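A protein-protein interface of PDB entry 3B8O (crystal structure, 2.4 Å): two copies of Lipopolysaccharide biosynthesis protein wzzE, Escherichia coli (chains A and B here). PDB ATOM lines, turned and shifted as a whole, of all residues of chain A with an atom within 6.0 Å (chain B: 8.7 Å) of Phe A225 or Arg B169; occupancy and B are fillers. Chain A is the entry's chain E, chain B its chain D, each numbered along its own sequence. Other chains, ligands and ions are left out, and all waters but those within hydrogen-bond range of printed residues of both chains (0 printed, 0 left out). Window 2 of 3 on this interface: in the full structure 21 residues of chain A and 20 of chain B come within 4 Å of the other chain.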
ATOM      1  N   GLN A 159     -11.501 -19.045  28.862  1.00  0.00           N
ATOM      2  CA  GLN A 159     -11.798 -17.688  29.310  1.00  0.00           C
ATOM      3  C   GLN A 159     -12.021 -16.761  28.120  1.00  0.00           C
ATOM      4  O   GLN A 159     -12.910 -15.900  28.144  1.00  0.00           O
ATOM      5  CB  GLN A 159     -10.710 -17.150  30.218  1.00  0.00           C
ATOM      6  CG  GLN A 159     -10.926 -17.459  31.675  1.00  0.00           C
ATOM      7  CD  GLN A 159      -9.790 -16.970  32.548  1.00  0.00           C
ATOM      8  OE1 GLN A 159      -9.982 -16.106  33.407  1.00  0.00           O
ATOM      9  NE2 GLN A 159      -8.599 -17.501  32.324  1.00  0.00           N
ATOM     10  N   GLU A 160     -11.219 -16.972  27.079  1.00  0.00           N
ATOM     11  CA  GLU A 160     -11.365 -16.242  25.816  1.00  0.00           C
ATOM     12  C   GLU A 160     -12.671 -16.565  25.105  1.00  0.00           C
ATOM     13  O   GLU A 160     -13.325 -15.659  24.605  1.00  0.00           O
ATOM     14  CB  GLU A 160     -10.184 -16.520  24.886  1.00  0.00           C
ATOM     15  CG  GLU A 160      -8.904 -15.845  25.310  1.00  0.00           C
ATOM     16  CD  GLU A 160      -7.667 -16.557  24.784  1.00  0.00           C
ATOM     17  OE1 GLU A 160      -7.792 -17.421  23.882  1.00  0.00           O
ATOM     18  OE2 GLU A 160      -6.565 -16.266  25.278  1.00  0.00           O
ATOM     19  N   ALA A 163     -15.559 -14.667  26.772  1.00  0.00           N
ATOM     20  CA  ALA A 163     -15.550 -13.257  26.417  1.00  0.00           C
ATOM     21  C   ALA A 163     -15.993 -13.035  24.977  1.00  0.00           C
ATOM     22  O   ALA A 163     -16.607 -12.013  24.666  1.00  0.00           O
ATOM     23  CB  ALA A 163     -14.182 -12.685  26.634  1.00  0.00           C
ATOM     24  N   VAL A 221     -12.272  -2.220  18.932  1.00  0.00           N
ATOM     25  CA  VAL A 221     -11.633  -2.687  20.173  1.00  0.00           C
ATOM     26  C   VAL A 221     -11.422  -4.201  20.145  1.00  0.00           C
ATOM     27  O   VAL A 221     -10.477  -4.668  19.506  1.00  0.00           O
ATOM     28  CB  VAL A 221     -12.376  -2.185  21.474  1.00  0.00           C
ATOM     29  CG1 VAL A 221     -13.762  -2.812  21.626  1.00  0.00           C
ATOM     30  CG2 VAL A 221     -11.545  -2.421  22.735  1.00  0.00           C
ATOM     31  N   PRO A 223     -12.991  -8.162  22.516  1.00  0.00           N
ATOM     32  CA  PRO A 223     -13.683  -8.700  23.701  1.00  0.00           C
ATOM     33  C   PRO A 223     -13.048  -8.235  25.018  1.00  0.00           C
ATOM     34  O   PRO A 223     -11.841  -8.013  25.064  1.00  0.00           O
ATOM     35  CB  PRO A 223     -13.541 -10.219  23.534  1.00  0.00           C
ATOM     36  CG  PRO A 223     -13.118 -10.435  22.083  1.00  0.00           C
ATOM     37  CD  PRO A 223     -12.335  -9.225  21.731  1.00  0.00           C
ATOM     38  N   ALA A 224     -13.862  -8.087  26.063  1.00  0.00           N
ATOM     39  CA  ALA A 224     -13.436  -7.530  27.348  1.00  0.00           C
ATOM     40  C   ALA A 224     -12.818  -8.595  28.246  1.00  0.00           C
ATOM     41  O   ALA A 224     -13.219  -9.761  28.209  1.00  0.00           O
ATOM     42  CB  ALA A 224     -14.612  -6.881  28.048  1.00  0.00           C
ATOM     43  N   PHE A 225     -11.855  -8.204  29.072  1.00  0.00           N
ATOM     44  CA  PHE A 225     -11.076  -9.195  29.813  1.00  0.00           C
ATOM     45  C   PHE A 225     -10.895  -8.857  31.286  1.00  0.00           C
ATOM     46  O   PHE A 225     -10.405  -7.773  31.635  1.00  0.00           O
ATOM     47  CB  PHE A 225      -9.731  -9.406  29.135  1.00  0.00           C
ATOM     48  CG  PHE A 225      -9.796 -10.326  27.953  1.00  0.00           C
ATOM     49  CD1 PHE A 225      -9.479  -9.866  26.682  1.00  0.00           C
ATOM     50  CD2 PHE A 225     -10.176 -11.660  28.110  1.00  0.00           C
ATOM     51  CE1 PHE A 225      -9.523 -10.715  25.583  1.00  0.00           C
ATOM     52  CE2 PHE A 225     -10.228 -12.524  27.019  1.00  0.00           C
ATOM     53  CZ  PHE A 225      -9.900 -12.041  25.745  1.00  0.00           C
ATOM     54  N   ASP A 226     -11.293  -9.787  32.153  1.00  0.00           N
ATOM     55  CA  ASP A 226     -11.161  -9.540  33.588  1.00  0.00           C
ATOM     56  C   ASP A 226      -9.746  -9.775  34.111  1.00  0.00           C
ATOM     57  O   ASP A 226      -8.949 -10.470  33.487  1.00  0.00           O
ATOM     58  CB  ASP A 226     -12.247 -10.249  34.438  1.00  0.00           C
ATOM     59  CG  ASP A 226     -12.233 -11.772  34.313  1.00  0.00           C
ATOM     60  OD1 ASP A 226     -13.137 -12.398  34.915  1.00  0.00           O
ATOM     61  OD2 ASP A 226     -11.350 -12.354  33.637  1.00  0.00           O
ATOM     62  N   LEU A 227      -9.448  -9.131  35.234  1.00  0.00           N
ATOM     63  CA  LEU A 227      -8.207  -9.296  35.969  1.00  0.00           C
ATOM     64  C   LEU A 227      -7.766 -10.750  36.016  1.00  0.00           C
ATOM     65  O   LEU A 227      -6.585 -11.075  35.823  1.00  0.00           O
ATOM     66  CB  LEU A 227      -8.423  -8.790  37.391  1.00  0.00           C
ATOM     67  CG  LEU A 227      -7.213  -8.546  38.287  1.00  0.00           C
ATOM     68  CD1 LEU A 227      -6.080  -7.908  37.507  1.00  0.00           C
ATOM     69  CD2 LEU A 227      -7.597  -7.693  39.501  1.00  0.00           C
ATOM     70  N   TYR A 229      -8.184 -13.046  33.953  1.00  0.00           N
ATOM     71  CA  TYR A 229      -7.625 -13.446  32.669  1.00  0.00           C
ATOM     72  C   TYR A 229      -6.159 -13.058  32.532  1.00  0.00           C
ATOM     73  O   TYR A 229      -5.326 -13.849  32.093  1.00  0.00           O
ATOM     74  CB  TYR A 229      -8.431 -12.833  31.515  1.00  0.00           C
ATOM     75  CG  TYR A 229      -7.843 -13.129  30.164  1.00  0.00           C
ATOM     76  CD1 TYR A 229      -7.999 -14.375  29.589  1.00  0.00           C
ATOM     77  CD2 TYR A 229      -7.117 -12.166  29.466  1.00  0.00           C
ATOM     78  CE1 TYR A 229      -7.462 -14.669  28.352  1.00  0.00           C
ATOM     79  CE2 TYR A 229      -6.567 -12.451  28.220  1.00  0.00           C
ATOM     80  CZ  TYR A 229      -6.748 -13.718  27.668  1.00  0.00           C
ATOM     81  OH  TYR A 229      -6.226 -14.037  26.439  1.00  0.00           O
ATOM     82  N   ASP A 230      -5.848 -11.822  32.885  1.00  0.00           N
ATOM     83  CA  ASP A 230      -4.501 -11.339  32.696  1.00  0.00           C
ATOM     84  C   ASP A 230      -3.578 -12.015  33.697  1.00  0.00           C
ATOM     85  O   ASP A 230      -2.469 -12.400  33.344  1.00  0.00           O
ATOM     86  CB  ASP A 230      -4.469  -9.823  32.753  1.00  0.00           C
ATOM     87  CG  ASP A 230      -5.166  -9.188  31.539  1.00  0.00           C
ATOM     88  OD1 ASP A 230      -4.791  -9.533  30.393  1.00  0.00           O
ATOM     89  OD2 ASP A 230      -6.084  -8.346  31.715  1.00  0.00           O
ATOM     90  N   VAL B 162       1.153  -8.004  34.272  1.00  0.00           N
ATOM     91  CA  VAL B 162      -0.308  -7.907  34.230  1.00  0.00           C
ATOM     92  C   VAL B 162      -0.780  -6.459  34.047  1.00  0.00           C
ATOM     93  O   VAL B 162      -1.661  -6.171  33.226  1.00  0.00           O
ATOM     94  CB  VAL B 162      -0.965  -8.503  35.501  1.00  0.00           C
ATOM     95  CG1 VAL B 162      -2.448  -8.173  35.558  1.00  0.00           C
ATOM     96  CG2 VAL B 162      -0.761 -10.002  35.546  1.00  0.00           C
ATOM     97  N   ALA B 163      -0.207  -5.545  34.820  1.00  0.00           N
ATOM     98  CA  ALA B 163      -0.570  -4.134  34.709  1.00  0.00           C
ATOM     99  C   ALA B 163      -0.190  -3.590  33.329  1.00  0.00           C
ATOM    100  O   ALA B 163      -0.874  -2.752  32.793  1.00  0.00           O
ATOM    101  CB  ALA B 163       0.092  -3.342  35.808  1.00  0.00           C
ATOM    102  N   LYS B 164       0.898  -4.111  32.764  1.00  0.00           N
ATOM    103  CA  LYS B 164       1.340  -3.802  31.405  1.00  0.00           C
ATOM    104  C   LYS B 164       0.336  -4.261  30.342  1.00  0.00           C
ATOM    105  O   LYS B 164       0.056  -3.532  29.388  1.00  0.00           O
ATOM    106  CB  LYS B 164       2.726  -4.414  31.148  1.00  0.00           C
ATOM    107  CG  LYS B 164       3.331  -4.161  29.762  1.00  0.00           C
ATOM    108  CD  LYS B 164       3.626  -2.672  29.525  1.00  0.00           C
ATOM    109  CE  LYS B 164       4.271  -2.414  28.155  1.00  0.00           C
ATOM    110  NZ  LYS B 164       4.297  -0.935  27.823  1.00  0.00           N
ATOM    111  N   ALA B 165      -0.196  -5.465  30.510  1.00  0.00           N
ATOM    112  CA  ALA B 165      -1.191  -5.988  29.595  1.00  0.00           C
ATOM    113  C   ALA B 165      -2.458  -5.139  29.663  1.00  0.00           C
ATOM    114  O   ALA B 165      -2.997  -4.750  28.623  1.00  0.00           O
ATOM    115  CB  ALA B 165      -1.491  -7.448  29.900  1.00  0.00           C
ATOM    116  N   ILE B 166      -2.902  -4.825  30.882  1.00  0.00           N
ATOM    117  CA  ILE B 166      -4.106  -4.015  31.096  1.00  0.00           C
ATOM    118  C   ILE B 166      -3.907  -2.593  30.545  1.00  0.00           C
ATOM    119  O   ILE B 166      -4.828  -1.988  29.989  1.00  0.00           O
ATOM    120  CB  ILE B 166      -4.531  -3.991  32.587  1.00  0.00           C
ATOM    121  CG1 ILE B 166      -4.932  -5.396  33.051  1.00  0.00           C
ATOM    122  CG2 ILE B 166      -5.712  -3.078  32.803  1.00  0.00           C
ATOM    123  CD1 ILE B 166      -5.156  -5.527  34.560  1.00  0.00           C
ATOM    124  N   TYR B 167      -2.689  -2.087  30.690  1.00  0.00           N
ATOM    125  CA  TYR B 167      -2.312  -0.787  30.178  1.00  0.00           C
ATOM    126  C   TYR B 167      -2.430  -0.706  28.647  1.00  0.00           C
ATOM    127  O   TYR B 167      -3.003   0.243  28.109  1.00  0.00           O
ATOM    128  CB  TYR B 167      -0.887  -0.486  30.603  1.00  0.00           C
ATOM    129  CG  TYR B 167      -0.314   0.791  30.055  1.00  0.00           C
ATOM    130  CD1 TYR B 167      -0.676   2.018  30.590  1.00  0.00           C
ATOM    131  CD2 TYR B 167       0.626   0.769  29.017  1.00  0.00           C
ATOM    132  CE1 TYR B 167      -0.137   3.184  30.107  1.00  0.00           C
ATOM    133  CE2 TYR B 167       1.176   1.944  28.523  1.00  0.00           C
ATOM    134  CZ  TYR B 167       0.790   3.153  29.080  1.00  0.00           C
ATOM    135  OH  TYR B 167       1.314   4.343  28.613  1.00  0.00           O
ATOM    136  N   ASP B 168      -1.868  -1.700  27.965  1.00  0.00           N
ATOM    137  CA  ASP B 168      -1.856  -1.738  26.509  1.00  0.00           C
ATOM    138  C   ASP B 168      -3.266  -1.897  25.972  1.00  0.00           C
ATOM    139  O   ASP B 168      -3.623  -1.277  24.972  1.00  0.00           O
ATOM    140  CB  ASP B 168      -0.965  -2.883  26.010  1.00  0.00           C
ATOM    141  CG  ASP B 168       0.508  -2.650  26.308  1.00  0.00           C
ATOM    142  OD1 ASP B 168       0.925  -1.465  26.352  1.00  0.00           O
ATOM    143  OD2 ASP B 168       1.243  -3.652  26.489  1.00  0.00           O
ATOM    144  N   ARG B 169      -4.052  -2.742  26.639  1.00  0.00           N
ATOM    145  CA  ARG B 169      -5.445  -2.958  26.298  1.00  0.00           C
ATOM    146  C   ARG B 169      -6.172  -1.622  26.317  1.00  0.00           C
ATOM    147  O   ARG B 169      -6.921  -1.307  25.396  1.00  0.00           O
ATOM    148  CB  ARG B 169      -6.085  -3.923  27.293  1.00  0.00           C
ATOM    149  CG  ARG B 169      -7.504  -4.347  26.930  1.00  0.00           C
ATOM    150  CD  ARG B 169      -7.925  -5.661  27.633  1.00  0.00           C
ATOM    151  NE  ARG B 169      -7.152  -6.822  27.192  1.00  0.00           N
ATOM    152  CZ  ARG B 169      -6.641  -7.737  28.013  1.00  0.00           C
ATOM    153  NH1 ARG B 169      -6.836  -7.633  29.318  1.00  0.00           N
ATOM    154  NH2 ARG B 169      -5.946  -8.768  27.531  1.00  0.00           N
ATOM    155  N   ARG B 170      -5.926  -0.844  27.374  1.00  0.00           N
ATOM    156  CA  ARG B 170      -6.527   0.467  27.570  1.00  0.00           C
ATOM    157  C   ARG B 170      -6.020   1.499  26.537  1.00  0.00           C
ATOM    158  O   ARG B 170      -6.742   2.432  26.165  1.00  0.00           O
ATOM    159  CB  ARG B 170      -6.225   0.943  28.992  1.00  0.00           C
ATOM    160  CG  ARG B 170      -7.186   1.976  29.553  1.00  0.00           C
ATOM    161  CD  ARG B 170      -8.431   1.331  30.172  1.00  0.00           C
ATOM    162  NE  ARG B 170      -9.596   2.209  30.065  1.00  0.00           N
ATOM    163  CZ  ARG B 170      -9.918   3.154  30.952  1.00  0.00           C
ATOM    164  NH1 ARG B 170      -9.168   3.359  32.038  1.00  0.00           N
ATOM    165  NH2 ARG B 170     -11.001   3.895  30.753  1.00  0.00           N
ATOM    166  N   MET B 171      -4.785   1.307  26.081  1.00  0.00           N
ATOM    167  CA  MET B 171      -4.110   2.230  25.193  1.00  0.00           C
ATOM    168  C   MET B 171      -4.671   2.151  23.785  1.00  0.00           C
ATOM    169  O   MET B 171      -4.922   3.174  23.150  1.00  0.00           O
ATOM    170  CB  MET B 171      -2.601   1.957  25.163  1.00  0.00           C
ATOM    171  CG  MET B 171      -1.830   2.996  24.348  1.00  0.00           C
ATOM    172  SD  MET B 171      -1.883   4.726  25.267  1.00  0.00           S
ATOM    173  CE  MET B 171      -0.113   4.590  26.064  1.00  0.00           C
ATOM    174  N   ASN B 172      -4.842   0.936  23.290  1.00  0.00           N
ATOM    175  CA  ASN B 172      -5.444   0.744  21.995  1.00  0.00           C
ATOM    176  C   ASN B 172      -6.862   1.303  22.012  1.00  0.00           C
ATOM    177  O   ASN B 172      -7.191   2.236  21.264  1.00  0.00           O
ATOM    178  CB  ASN B 172      -5.445  -0.736  21.623  1.00  0.00           C
ATOM    179  CG  ASN B 172      -6.284  -1.023  20.400  1.00  0.00           C
ATOM    180  OD1 ASN B 172      -6.391  -0.189  19.498  1.00  0.00           O
ATOM    181  ND2 ASN B 172      -6.878  -2.215  20.354  1.00  0.00           N
ATOM    182  N   SER B 173      -7.681   0.765  22.909  1.00  0.00           N
ATOM    183  CA  SER B 173      -9.082   1.161  23.021  1.00  0.00           C
ATOM    184  C   SER B 173      -9.326   2.686  22.971  1.00  0.00           C
ATOM    185  O   SER B 173     -10.282   3.136  22.330  1.00  0.00           O
ATOM    186  CB  SER B 173      -9.701   0.563  24.282  1.00  0.00           C
ATOM    187  OG  SER B 173      -8.949   0.923  25.418  1.00  0.00           O
ATOM    188  N   ILE B 174      -8.466   3.467  23.637  1.00  0.00           N
ATOM    189  CA  ILE B 174      -8.619   4.929  23.692  1.00  0.00           C
ATOM    190  C   ILE B 174      -8.308   5.596  22.359  1.00  0.00           C
ATOM    191  O   ILE B 174      -9.006   6.527  21.956  1.00  0.00           O
ATOM    192  CB  ILE B 174      -7.812   5.581  24.845  1.00  0.00           C
ATOM    193  CG1 ILE B 174      -8.611   5.517  26.146  1.00  0.00           C
ATOM    194  CG2 ILE B 174      -7.517   7.047  24.538  1.00  0.00           C
ATOM    195  CD1 ILE B 174      -7.903   6.152  27.349  1.00  0.00           C
ATOM    196  N   GLU B 175      -7.278   5.114  21.671  1.00  0.00           N
ATOM    197  CA  GLU B 175      -6.936   5.671  20.364  1.00  0.00           C
ATOM    198  C   GLU B 175      -8.086   5.470  19.387  1.00  0.00           C
ATOM    199  O   GLU B 175      -8.508   6.406  18.660  1.00  0.00           O
ATOM    200  CB  GLU B 175      -5.663   5.030  19.819  1.00  0.00           C
ATOM    201  CG  GLU B 175      -4.380   5.501  20.500  1.00  0.00           C
ATOM    202  CD  GLU B 175      -3.146   4.813  19.944  1.00  0.00           C
ATOM    203  OE1 GLU B 175      -2.452   5.419  19.096  1.00  0.00           O
ATOM    204  OE2 GLU B 175      -2.887   3.657  20.334  1.00  0.00           O
ATOM    205  N   GLN B 176      -8.618   4.251  19.403  1.00  0.00           N
ATOM    206  CA  GLN B 176      -9.583   3.831  18.394  1.00  0.00           C
ATOM    207  C   GLN B 176     -11.004   4.402  18.576  1.00  0.00           C
ATOM    208  O   GLN B 176     -11.237   5.249  19.538  1.00  0.00           O
ATOM    209  CB  GLN B 176      -9.565   2.303  18.285  1.00  0.00           C
ATOM    210  CG  GLN B 176      -8.310   1.790  17.590  1.00  0.00           C
ATOM    211  CD  GLN B 176      -8.427   0.343  17.156  1.00  0.00           C
ATOM    212  OE1 GLN B 176      -8.541  -0.550  17.984  1.00  0.00           O
ATOM    213  NE2 GLN B 176      -8.387   0.105  15.850  1.00  0.00           N
ATOM    214  N   LEU B 218      -2.705   8.857  29.897  1.00  0.00           N
ATOM    215  CA  LEU B 218      -2.358   7.448  30.076  1.00  0.00           C
ATOM    216  C   LEU B 218      -0.905   7.162  29.694  1.00  0.00           C
ATOM    217  O   LEU B 218      -0.208   6.396  30.372  1.00  0.00           O
ATOM    218  CB  LEU B 218      -3.300   6.574  29.231  1.00  0.00           C
ATOM    219  CG  LEU B 218      -3.268   5.051  29.455  1.00  0.00           C
ATOM    220  CD1 LEU B 218      -4.184   4.624  30.604  1.00  0.00           C
ATOM    221  CD2 LEU B 218      -3.643   4.334  28.175  1.00  0.00           C
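The guanidinium group (NH1) of Arg B169 lies within salt-bridge range of the side-chain carboxylate (OD2) of Asp A230 (2.6 Å).
The side-chain hydroxyl (OH) of Tyr A229 is in hydrogen-bond range of the side-chain carboxylate (OE2) of Glu A160, 2.5 Å away.
O of Arg B170 sits at hydrogen-bond distance from OG of Ser B173 (2.8 Å).
OD2 of Asp A226 sits at hydrogen-bond distance from N of Tyr A229 (3.3 Å).
The side-chain hydroxyl of Ser B173 lies within hydrogen-bond range of the backbone carbonyl oxygen of Arg B169 (3.0 Å).
Among the printed residues, pairs that only touch across the chains: Val A221 with Ser B173 (3.8 Å), Phe A225 with Arg B169 (3.4 Å), Leu A227 with Ile B166 (3.9 Å), Tyr A229 with Arg B169 (3.8 Å), Asp A230 with Val B162 (3.7 Å), Asp A230 with Ala B165 (3.9 Å) and Asp A230 with Ile B166 (3.4 Å).
No residue of chain B comes within 4 Å of Ala A224.
Of chain B, only Arg B169 (3.4 Å) comes within 4 Å of Phe A225.
Printed residues of chain B within 4 Å of Leu A227: Ile B166.
Of the printed residues of chain B, Tyr A229 touches Arg B169 (3.8 Å).
Of the printed residues of chain A, Val B162 touches Asp A230.
Printed residues of chain A within 4 Å of Ala B165: Asp A230.
Tyr B167 touches none of the printed residues of chain A.
Arg B169 touches just these residues of chain A: Phe A225 (3.4 Å), Tyr A229 (3.8 Å) and Asp A230 (2.6 Å).
The nearest residue of chain A that does not touch Arg B169 is Pro A223 (5.2 Å).
Of the 16 printed residues of chain B, 5 touch a printed residue of chain A.
Of the 11 printed residues of chain A, 5 touch a printed residue of chain B.
Among the printed residues, 8 pairs touch across the chains.
1 position is printed for both chains.
Of the 8 pairs that touch across the chains among the printed residues, none has its exchanged pair printed and touching as well.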
